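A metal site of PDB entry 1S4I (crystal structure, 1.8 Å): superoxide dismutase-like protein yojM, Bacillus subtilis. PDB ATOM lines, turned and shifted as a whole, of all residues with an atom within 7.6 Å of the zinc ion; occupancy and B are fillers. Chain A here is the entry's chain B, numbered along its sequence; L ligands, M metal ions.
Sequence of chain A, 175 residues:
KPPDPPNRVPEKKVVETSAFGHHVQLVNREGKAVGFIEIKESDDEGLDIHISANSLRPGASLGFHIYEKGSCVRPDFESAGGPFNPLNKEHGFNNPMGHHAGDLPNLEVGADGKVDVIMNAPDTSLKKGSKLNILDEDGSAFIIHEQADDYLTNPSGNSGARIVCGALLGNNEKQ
The zinc ion is bound by OD2 of Asp 103, CL1 of the ligand, ND1 of His 100 and ND1 of His 91.
The zinc ion has four donor atoms within binding distance.
The backbone NH of Gly 92 lies within hydrogen-bond range of the side-chain carboxylate of Asp 103 (3.0 Å).
NE2 of His 100 lies close to O of Lys 89 (3.4 Å).
A ring nitrogen (ND1) of His 91 sits close to the backbone carbonyl oxygen (O) of Pro 155, at 3.3 Å.
OD1 of Asn 154 sits at hydrogen-bond distance from N of His 91 (2.9 Å).
The backbone NH (N) of His 100 lies within hydrogen-bond range of the backbone carbonyl oxygen (O) of Glu 90 (3.3 Å).
NE2 of His 91 sits close to N of Gly 157, 3.4 Å away.
A ring nitrogen (NE2) of His 91 lies within hydrogen-bond range of the side-chain carboxylate (OD1) of Asp 149, 2.7 Å away.
Merely in contact with the zinc ion: Pro 155.
Of the 24 residues printed, 4 come within 4 Å of the zinc ion.
The nearest printed residue that does not touch the zinc ion is Pro 83 (4.3 Å).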
ATOM      1  N   PHE A  64     -16.744 -29.268  14.797  1.00  0.00           N
ATOM      2  CA  PHE A  64     -16.309 -28.740  13.482  1.00  0.00           C
ATOM      3  C   PHE A  64     -16.168 -27.221  13.730  1.00  0.00           C
ATOM      4  O   PHE A  64     -17.128 -26.658  14.068  1.00  0.00           O
ATOM      5  CB  PHE A  64     -17.421 -28.939  12.467  1.00  0.00           C
ATOM      6  CG  PHE A  64     -17.206 -28.321  11.043  1.00  0.00           C
ATOM      7  CD1 PHE A  64     -15.991 -28.395  10.319  1.00  0.00           C
ATOM      8  CD2 PHE A  64     -18.325 -27.817  10.386  1.00  0.00           C
ATOM      9  CE1 PHE A  64     -15.927 -27.876   8.957  1.00  0.00           C
ATOM     10  CE2 PHE A  64     -18.278 -27.298   9.040  1.00  0.00           C
ATOM     11  CZ  PHE A  64     -17.088 -27.249   8.399  1.00  0.00           C
ATOM     12  N   HIS A  65     -14.991 -26.664  13.570  1.00  0.00           N
ATOM     13  CA  HIS A  65     -14.685 -25.253  13.915  1.00  0.00           C
ATOM     14  C   HIS A  65     -13.774 -24.592  12.929  1.00  0.00           C
ATOM     15  O   HIS A  65     -13.056 -25.201  12.156  1.00  0.00           O
ATOM     16  CB  HIS A  65     -14.187 -24.994  15.393  1.00  0.00           C
ATOM     17  CG  HIS A  65     -14.798 -25.898  16.434  1.00  0.00           C
ATOM     18  ND1 HIS A  65     -14.026 -26.673  17.246  1.00  0.00           N
ATOM     19  CD2 HIS A  65     -16.095 -26.204  16.731  1.00  0.00           C
ATOM     20  CE1 HIS A  65     -14.802 -27.406  18.038  1.00  0.00           C
ATOM     21  NE2 HIS A  65     -16.059 -27.171  17.718  1.00  0.00           N
ATOM     22  N   ILE A  66     -13.804 -23.270  12.948  1.00  0.00           N
ATOM     23  CA  ILE A  66     -12.832 -22.487  12.099  1.00  0.00           C
ATOM     24  C   ILE A  66     -11.752 -21.988  13.050  1.00  0.00           C
ATOM     25  O   ILE A  66     -12.033 -21.435  14.177  1.00  0.00           O
ATOM     26  CB  ILE A  66     -13.586 -21.240  11.463  1.00  0.00           C
ATOM     27  CG1 ILE A  66     -14.782 -21.748  10.682  1.00  0.00           C
ATOM     28  CG2 ILE A  66     -12.595 -20.403  10.622  1.00  0.00           C
ATOM     29  CD1 ILE A  66     -15.557 -20.610   9.860  1.00  0.00           C
ATOM     30  N   TYR A  67     -10.497 -22.240  12.644  1.00  0.00           N
ATOM     31  CA  TYR A  67      -9.325 -21.936  13.449  1.00  0.00           C
ATOM     32  C   TYR A  67      -8.583 -20.811  12.737  1.00  0.00           C
ATOM     33  O   TYR A  67      -8.808 -20.569  11.507  1.00  0.00           O
ATOM     34  CB  TYR A  67      -8.453 -23.227  13.603  1.00  0.00           C
ATOM     35  CG  TYR A  67      -9.145 -24.212  14.561  1.00  0.00           C
ATOM     36  CD1 TYR A  67      -8.888 -24.166  15.954  1.00  0.00           C
ATOM     37  CD2 TYR A  67     -10.153 -25.090  14.097  1.00  0.00           C
ATOM     38  CE1 TYR A  67      -9.528 -25.015  16.847  1.00  0.00           C
ATOM     39  CE2 TYR A  67     -10.786 -25.928  14.990  1.00  0.00           C
ATOM     40  CZ  TYR A  67     -10.461 -25.908  16.349  1.00  0.00           C
ATOM     41  OH  TYR A  67     -11.157 -26.703  17.213  1.00  0.00           O
ATOM     42  N   PRO A  83      -8.850 -21.262  18.011  1.00  0.00           N
ATOM     43  CA  PRO A  83     -10.128 -20.766  17.455  1.00  0.00           C
ATOM     44  C   PRO A  83     -10.181 -19.403  16.810  1.00  0.00           C
ATOM     45  O   PRO A  83      -9.594 -18.452  17.269  1.00  0.00           O
ATOM     46  CB  PRO A  83     -11.142 -20.937  18.619  1.00  0.00           C
ATOM     47  CG  PRO A  83     -10.362 -21.601  19.755  1.00  0.00           C
ATOM     48  CD  PRO A  83      -8.929 -21.536  19.457  1.00  0.00           C
ATOM     49  N   PHE A  84     -10.888 -19.325  15.704  1.00  0.00           N
ATOM     50  CA  PHE A  84     -11.131 -18.008  15.123  1.00  0.00           C
ATOM     51  C   PHE A  84     -12.061 -17.277  16.053  1.00  0.00           C
ATOM     52  O   PHE A  84     -13.203 -17.670  16.238  1.00  0.00           O
ATOM     53  CB  PHE A  84     -11.742 -18.123  13.737  1.00  0.00           C
ATOM     54  CG  PHE A  84     -12.050 -16.809  13.097  1.00  0.00           C
ATOM     55  CD1 PHE A  84     -13.354 -16.423  12.847  1.00  0.00           C
ATOM     56  CD2 PHE A  84     -11.011 -15.960  12.718  1.00  0.00           C
ATOM     57  CE1 PHE A  84     -13.588 -15.132  12.180  1.00  0.00           C
ATOM     58  CE2 PHE A  84     -11.267 -14.722  12.078  1.00  0.00           C
ATOM     59  CZ  PHE A  84     -12.509 -14.331  11.857  1.00  0.00           C
ATOM     60  N   ASN A  85     -11.553 -16.228  16.712  1.00  0.00           N
ATOM     61  CA  ASN A  85     -12.257 -15.683  17.875  1.00  0.00           C
ATOM     62  C   ASN A  85     -11.982 -14.166  17.990  1.00  0.00           C
ATOM     63  O   ASN A  85     -11.475 -13.733  19.009  1.00  0.00           O
ATOM     64  CB  ASN A  85     -11.866 -16.435  19.178  1.00  0.00           C
ATOM     65  CG  ASN A  85     -12.700 -16.000  20.405  1.00  0.00           C
ATOM     66  OD1 ASN A  85     -13.811 -15.480  20.247  1.00  0.00           O
ATOM     67  ND2 ASN A  85     -12.143 -16.220  21.649  1.00  0.00           N
ATOM     68  N   LYS A  89     -14.549 -14.351  22.851  1.00  0.00           N
ATOM     69  CA  LYS A  89     -15.614 -14.891  23.689  1.00  0.00           C
ATOM     70  C   LYS A  89     -15.084 -16.197  24.164  1.00  0.00           C
ATOM     71  O   LYS A  89     -13.984 -16.592  23.792  1.00  0.00           O
ATOM     72  CB  LYS A  89     -16.862 -15.064  22.823  1.00  0.00           C
ATOM     73  CG  LYS A  89     -17.040 -13.826  21.965  1.00  0.00           C
ATOM     74  CD  LYS A  89     -18.464 -13.680  21.497  1.00  0.00           C
ATOM     75  CE  LYS A  89     -19.432 -13.524  22.655  1.00  0.00           C
ATOM     76  NZ  LYS A  89     -19.511 -12.046  23.057  1.00  0.00           N
ATOM     77  N   GLU A  90     -15.823 -16.911  25.000  1.00  0.00           N
ATOM     78  CA  GLU A  90     -15.324 -18.258  25.142  1.00  0.00           C
ATOM     79  C   GLU A  90     -16.135 -19.223  24.210  1.00  0.00           C
ATOM     80  O   GLU A  90     -17.017 -18.745  23.460  1.00  0.00           O
ATOM     81  CB  GLU A  90     -15.217 -18.719  26.560  1.00  0.00           C
ATOM     82  CG  GLU A  90     -16.487 -18.826  27.322  1.00  0.00           C
ATOM     83  CD  GLU A  90     -16.215 -18.647  28.813  1.00  0.00           C
ATOM     84  OE1 GLU A  90     -16.287 -19.649  29.541  1.00  0.00           O
ATOM     85  OE2 GLU A  90     -15.947 -17.502  29.268  1.00  0.00           O
ATOM     86  N   HIS A  91     -15.861 -20.520  24.307  1.00  0.00           N
ATOM     87  CA  HIS A  91     -16.474 -21.563  23.481  1.00  0.00           C
ATOM     88  C   HIS A  91     -17.925 -21.922  23.764  1.00  0.00           C
ATOM     89  O   HIS A  91     -18.304 -22.185  24.919  1.00  0.00           O
ATOM     90  CB  HIS A  91     -15.674 -22.884  23.588  1.00  0.00           C
ATOM     91  CG  HIS A  91     -16.191 -23.966  22.662  1.00  0.00           C
ATOM     92  ND1 HIS A  91     -15.899 -23.987  21.316  1.00  0.00           N
ATOM     93  CD2 HIS A  91     -17.081 -24.967  22.871  1.00  0.00           C
ATOM     94  CE1 HIS A  91     -16.551 -24.995  20.741  1.00  0.00           C
ATOM     95  NE2 HIS A  91     -17.265 -25.622  21.665  1.00  0.00           N
ATOM     96  N   GLY A  92     -18.700 -22.042  22.688  1.00  0.00           N
ATOM     97  CA  GLY A  92     -19.881 -22.854  22.682  1.00  0.00           C
ATOM     98  C   GLY A  92     -21.204 -22.161  22.601  1.00  0.00           C
ATOM     99  O   GLY A  92     -21.443 -21.199  23.375  1.00  0.00           O
ATOM    100  N   PHE A  93     -22.101 -22.690  21.755  1.00  0.00           N
ATOM    101  CA  PHE A  93     -23.457 -22.178  21.644  1.00  0.00           C
ATOM    102  C   PHE A  93     -24.159 -22.149  23.032  1.00  0.00           C
ATOM    103  O   PHE A  93     -24.913 -21.221  23.322  1.00  0.00           O
ATOM    104  CB  PHE A  93     -24.320 -22.917  20.577  1.00  0.00           C
ATOM    105  CG  PHE A  93     -23.704 -22.948  19.197  1.00  0.00           C
ATOM    106  CD1 PHE A  93     -23.560 -24.137  18.533  1.00  0.00           C
ATOM    107  CD2 PHE A  93     -23.217 -21.797  18.612  1.00  0.00           C
ATOM    108  CE1 PHE A  93     -22.929 -24.190  17.294  1.00  0.00           C
ATOM    109  CE2 PHE A  93     -22.608 -21.814  17.371  1.00  0.00           C
ATOM    110  CZ  PHE A  93     -22.475 -23.077  16.706  1.00  0.00           C
ATOM    111  N   HIS A  99     -19.359 -17.257  22.769  1.00  0.00           N
ATOM    112  CA  HIS A  99     -19.607 -17.793  21.451  1.00  0.00           C
ATOM    113  C   HIS A  99     -18.425 -17.535  20.518  1.00  0.00           C
ATOM    114  O   HIS A  99     -18.347 -16.424  19.992  1.00  0.00           O
ATOM    115  CB  HIS A  99     -20.872 -17.082  20.987  1.00  0.00           C
ATOM    116  CG  HIS A  99     -21.549 -17.698  19.792  1.00  0.00           C
ATOM    117  ND1 HIS A  99     -22.868 -18.094  19.827  1.00  0.00           N
ATOM    118  CD2 HIS A  99     -21.124 -17.849  18.512  1.00  0.00           C
ATOM    119  CE1 HIS A  99     -23.225 -18.472  18.619  1.00  0.00           C
ATOM    120  NE2 HIS A  99     -22.193 -18.299  17.799  1.00  0.00           N
ATOM    121  N   HIS A 100     -17.489 -18.466  20.251  1.00  0.00           N
ATOM    122  CA  HIS A 100     -16.489 -18.060  19.240  1.00  0.00           C
ATOM    123  C   HIS A 100     -17.138 -17.922  17.878  1.00  0.00           C
ATOM    124  O   HIS A 100     -18.035 -18.713  17.556  1.00  0.00           O
ATOM    125  CB  HIS A 100     -15.358 -19.016  19.033  1.00  0.00           C
ATOM    126  CG  HIS A 100     -14.627 -19.394  20.289  1.00  0.00           C
ATOM    127  ND1 HIS A 100     -14.269 -20.719  20.557  1.00  0.00           N
ATOM    128  CD2 HIS A 100     -14.114 -18.658  21.300  1.00  0.00           C
ATOM    129  CE1 HIS A 100     -13.579 -20.765  21.691  1.00  0.00           C
ATOM    130  NE2 HIS A 100     -13.442 -19.525  22.150  1.00  0.00           N
ATOM    131  N   ALA A 101     -16.651 -16.969  17.068  1.00  0.00           N
ATOM    132  CA  ALA A 101     -17.171 -16.741  15.734  1.00  0.00           C
ATOM    133  C   ALA A 101     -16.936 -17.992  14.801  1.00  0.00           C
ATOM    134  O   ALA A 101     -17.656 -18.185  13.846  1.00  0.00           O
ATOM    135  CB  ALA A 101     -16.448 -15.546  15.119  1.00  0.00           C
ATOM    136  N   GLY A 102     -15.897 -18.719  15.110  1.00  0.00           N
ATOM    137  CA  GLY A 102     -15.523 -19.947  14.351  1.00  0.00           C
ATOM    138  C   GLY A 102     -16.208 -21.245  14.827  1.00  0.00           C
ATOM    139  O   GLY A 102     -15.970 -22.360  14.269  1.00  0.00           O
ATOM    140  N   ASP A 103     -17.067 -21.148  15.823  1.00  0.00           N
ATOM    141  CA  ASP A 103     -17.890 -22.259  16.260  1.00  0.00           C
ATOM    142  C   ASP A 103     -19.019 -22.587  15.320  1.00  0.00           C
ATOM    143  O   ASP A 103     -19.881 -21.747  15.055  1.00  0.00           O
ATOM    144  CB  ASP A 103     -18.500 -22.023  17.667  1.00  0.00           C
ATOM    145  CG  ASP A 103     -17.479 -22.026  18.738  1.00  0.00           C
ATOM    146  OD1 ASP A 103     -17.828 -21.614  19.873  1.00  0.00           O
ATOM    147  OD2 ASP A 103     -16.297 -22.425  18.553  1.00  0.00           O
ATOM    148  N   LEU A 104     -19.059 -23.837  14.818  1.00  0.00           N
ATOM    149  CA  LEU A 104     -20.046 -24.316  13.917  1.00  0.00           C
ATOM    150  C   LEU A 104     -20.752 -25.560  14.517  1.00  0.00           C
ATOM    151  O   LEU A 104     -20.168 -26.196  15.391  1.00  0.00           O
ATOM    152  CB  LEU A 104     -19.386 -24.701  12.563  1.00  0.00           C
ATOM    153  CG  LEU A 104     -18.474 -23.657  11.816  1.00  0.00           C
ATOM    154  CD1 LEU A 104     -17.923 -24.128  10.440  1.00  0.00           C
ATOM    155  CD2 LEU A 104     -19.125 -22.234  11.600  1.00  0.00           C
ATOM    156  N   ASP A 149     -18.801 -31.984  19.784  1.00  0.00           N
ATOM    157  CA  ASP A 149     -18.556 -30.790  20.544  1.00  0.00           C
ATOM    158  C   ASP A 149     -19.720 -30.744  21.488  1.00  0.00           C
ATOM    159  O   ASP A 149     -20.838 -31.054  21.088  1.00  0.00           O
ATOM    160  CB  ASP A 149     -18.586 -29.632  19.497  1.00  0.00           C
ATOM    161  CG  ASP A 149     -18.356 -28.224  20.108  1.00  0.00           C
ATOM    162  OD1 ASP A 149     -18.580 -27.970  21.337  1.00  0.00           O
ATOM    163  OD2 ASP A 149     -17.971 -27.299  19.341  1.00  0.00           O
ATOM    164  N   THR A 153     -17.845 -26.645  26.985  1.00  0.00           N
ATOM    165  CA  THR A 153     -16.487 -26.649  27.579  1.00  0.00           C
ATOM    166  C   THR A 153     -15.473 -25.873  26.740  1.00  0.00           C
ATOM    167  O   THR A 153     -15.460 -25.958  25.512  1.00  0.00           O
ATOM    168  CB  THR A 153     -15.993 -28.111  27.664  1.00  0.00           C
ATOM    169  OG1 THR A 153     -17.005 -28.882  28.323  1.00  0.00           O
ATOM    170  CG2 THR A 153     -14.810 -28.264  28.503  1.00  0.00           C
ATOM    171  N   ASN A 154     -14.602 -25.139  27.425  1.00  0.00           N
ATOM    172  CA  ASN A 154     -13.494 -24.467  26.752  1.00  0.00           C
ATOM    173  C   ASN A 154     -12.250 -25.342  26.596  1.00  0.00           C
ATOM    174  O   ASN A 154     -12.076 -26.192  27.444  1.00  0.00           O
ATOM    175  CB  ASN A 154     -13.082 -23.296  27.627  1.00  0.00           C
ATOM    176  CG  ASN A 154     -13.944 -22.177  27.423  1.00  0.00           C
ATOM    177  OD1 ASN A 154     -14.030 -21.684  26.291  1.00  0.00           O
ATOM    178  ND2 ASN A 154     -14.663 -21.749  28.493  1.00  0.00           N
ATOM    179  N   PRO A 155     -11.353 -25.115  25.606  1.00  0.00           N
ATOM    180  CA  PRO A 155     -11.518 -24.170  24.479  1.00  0.00           C
ATOM    181  C   PRO A 155     -12.364 -24.616  23.289  1.00  0.00           C
ATOM    182  O   PRO A 155     -12.843 -23.788  22.446  1.00  0.00           O
ATOM    183  CB  PRO A 155     -10.049 -23.931  23.979  1.00  0.00           C
ATOM    184  CG  PRO A 155      -9.277 -25.185  24.349  1.00  0.00           C
ATOM    185  CD  PRO A 155     -10.009 -25.768  25.590  1.00  0.00           C
ATOM    186  N   SER A 156     -12.541 -25.922  23.198  1.00  0.00           N
ATOM    187  CA  SER A 156     -13.134 -26.511  22.010  1.00  0.00           C
ATOM    188  C   SER A 156     -14.265 -27.535  22.226  1.00  0.00           C
ATOM    189  O   SER A 156     -14.536 -28.356  21.315  1.00  0.00           O
ATOM    190  CB  SER A 156     -12.019 -27.185  21.201  1.00  0.00           C
ATOM    191  OG  SER A 156     -12.124 -28.582  21.431  1.00  0.00           O
ATOM    192  N   GLY A 157     -14.938 -27.472  23.373  1.00  0.00           N
ATOM    193  CA  GLY A 157     -16.178 -28.203  23.511  1.00  0.00           C
ATOM    194  C   GLY A 157     -15.931 -29.678  23.805  1.00  0.00           C
ATOM    195  O   GLY A 157     -16.829 -30.525  23.664  1.00  0.00           O
HETATM  196 CL1  LIG L   1     -13.532 -23.887  18.959  1.00  0.00          CL
HETATM  197 ZN    ZN M   1     -14.910 -22.651  19.883  1.00  0.00          ZN
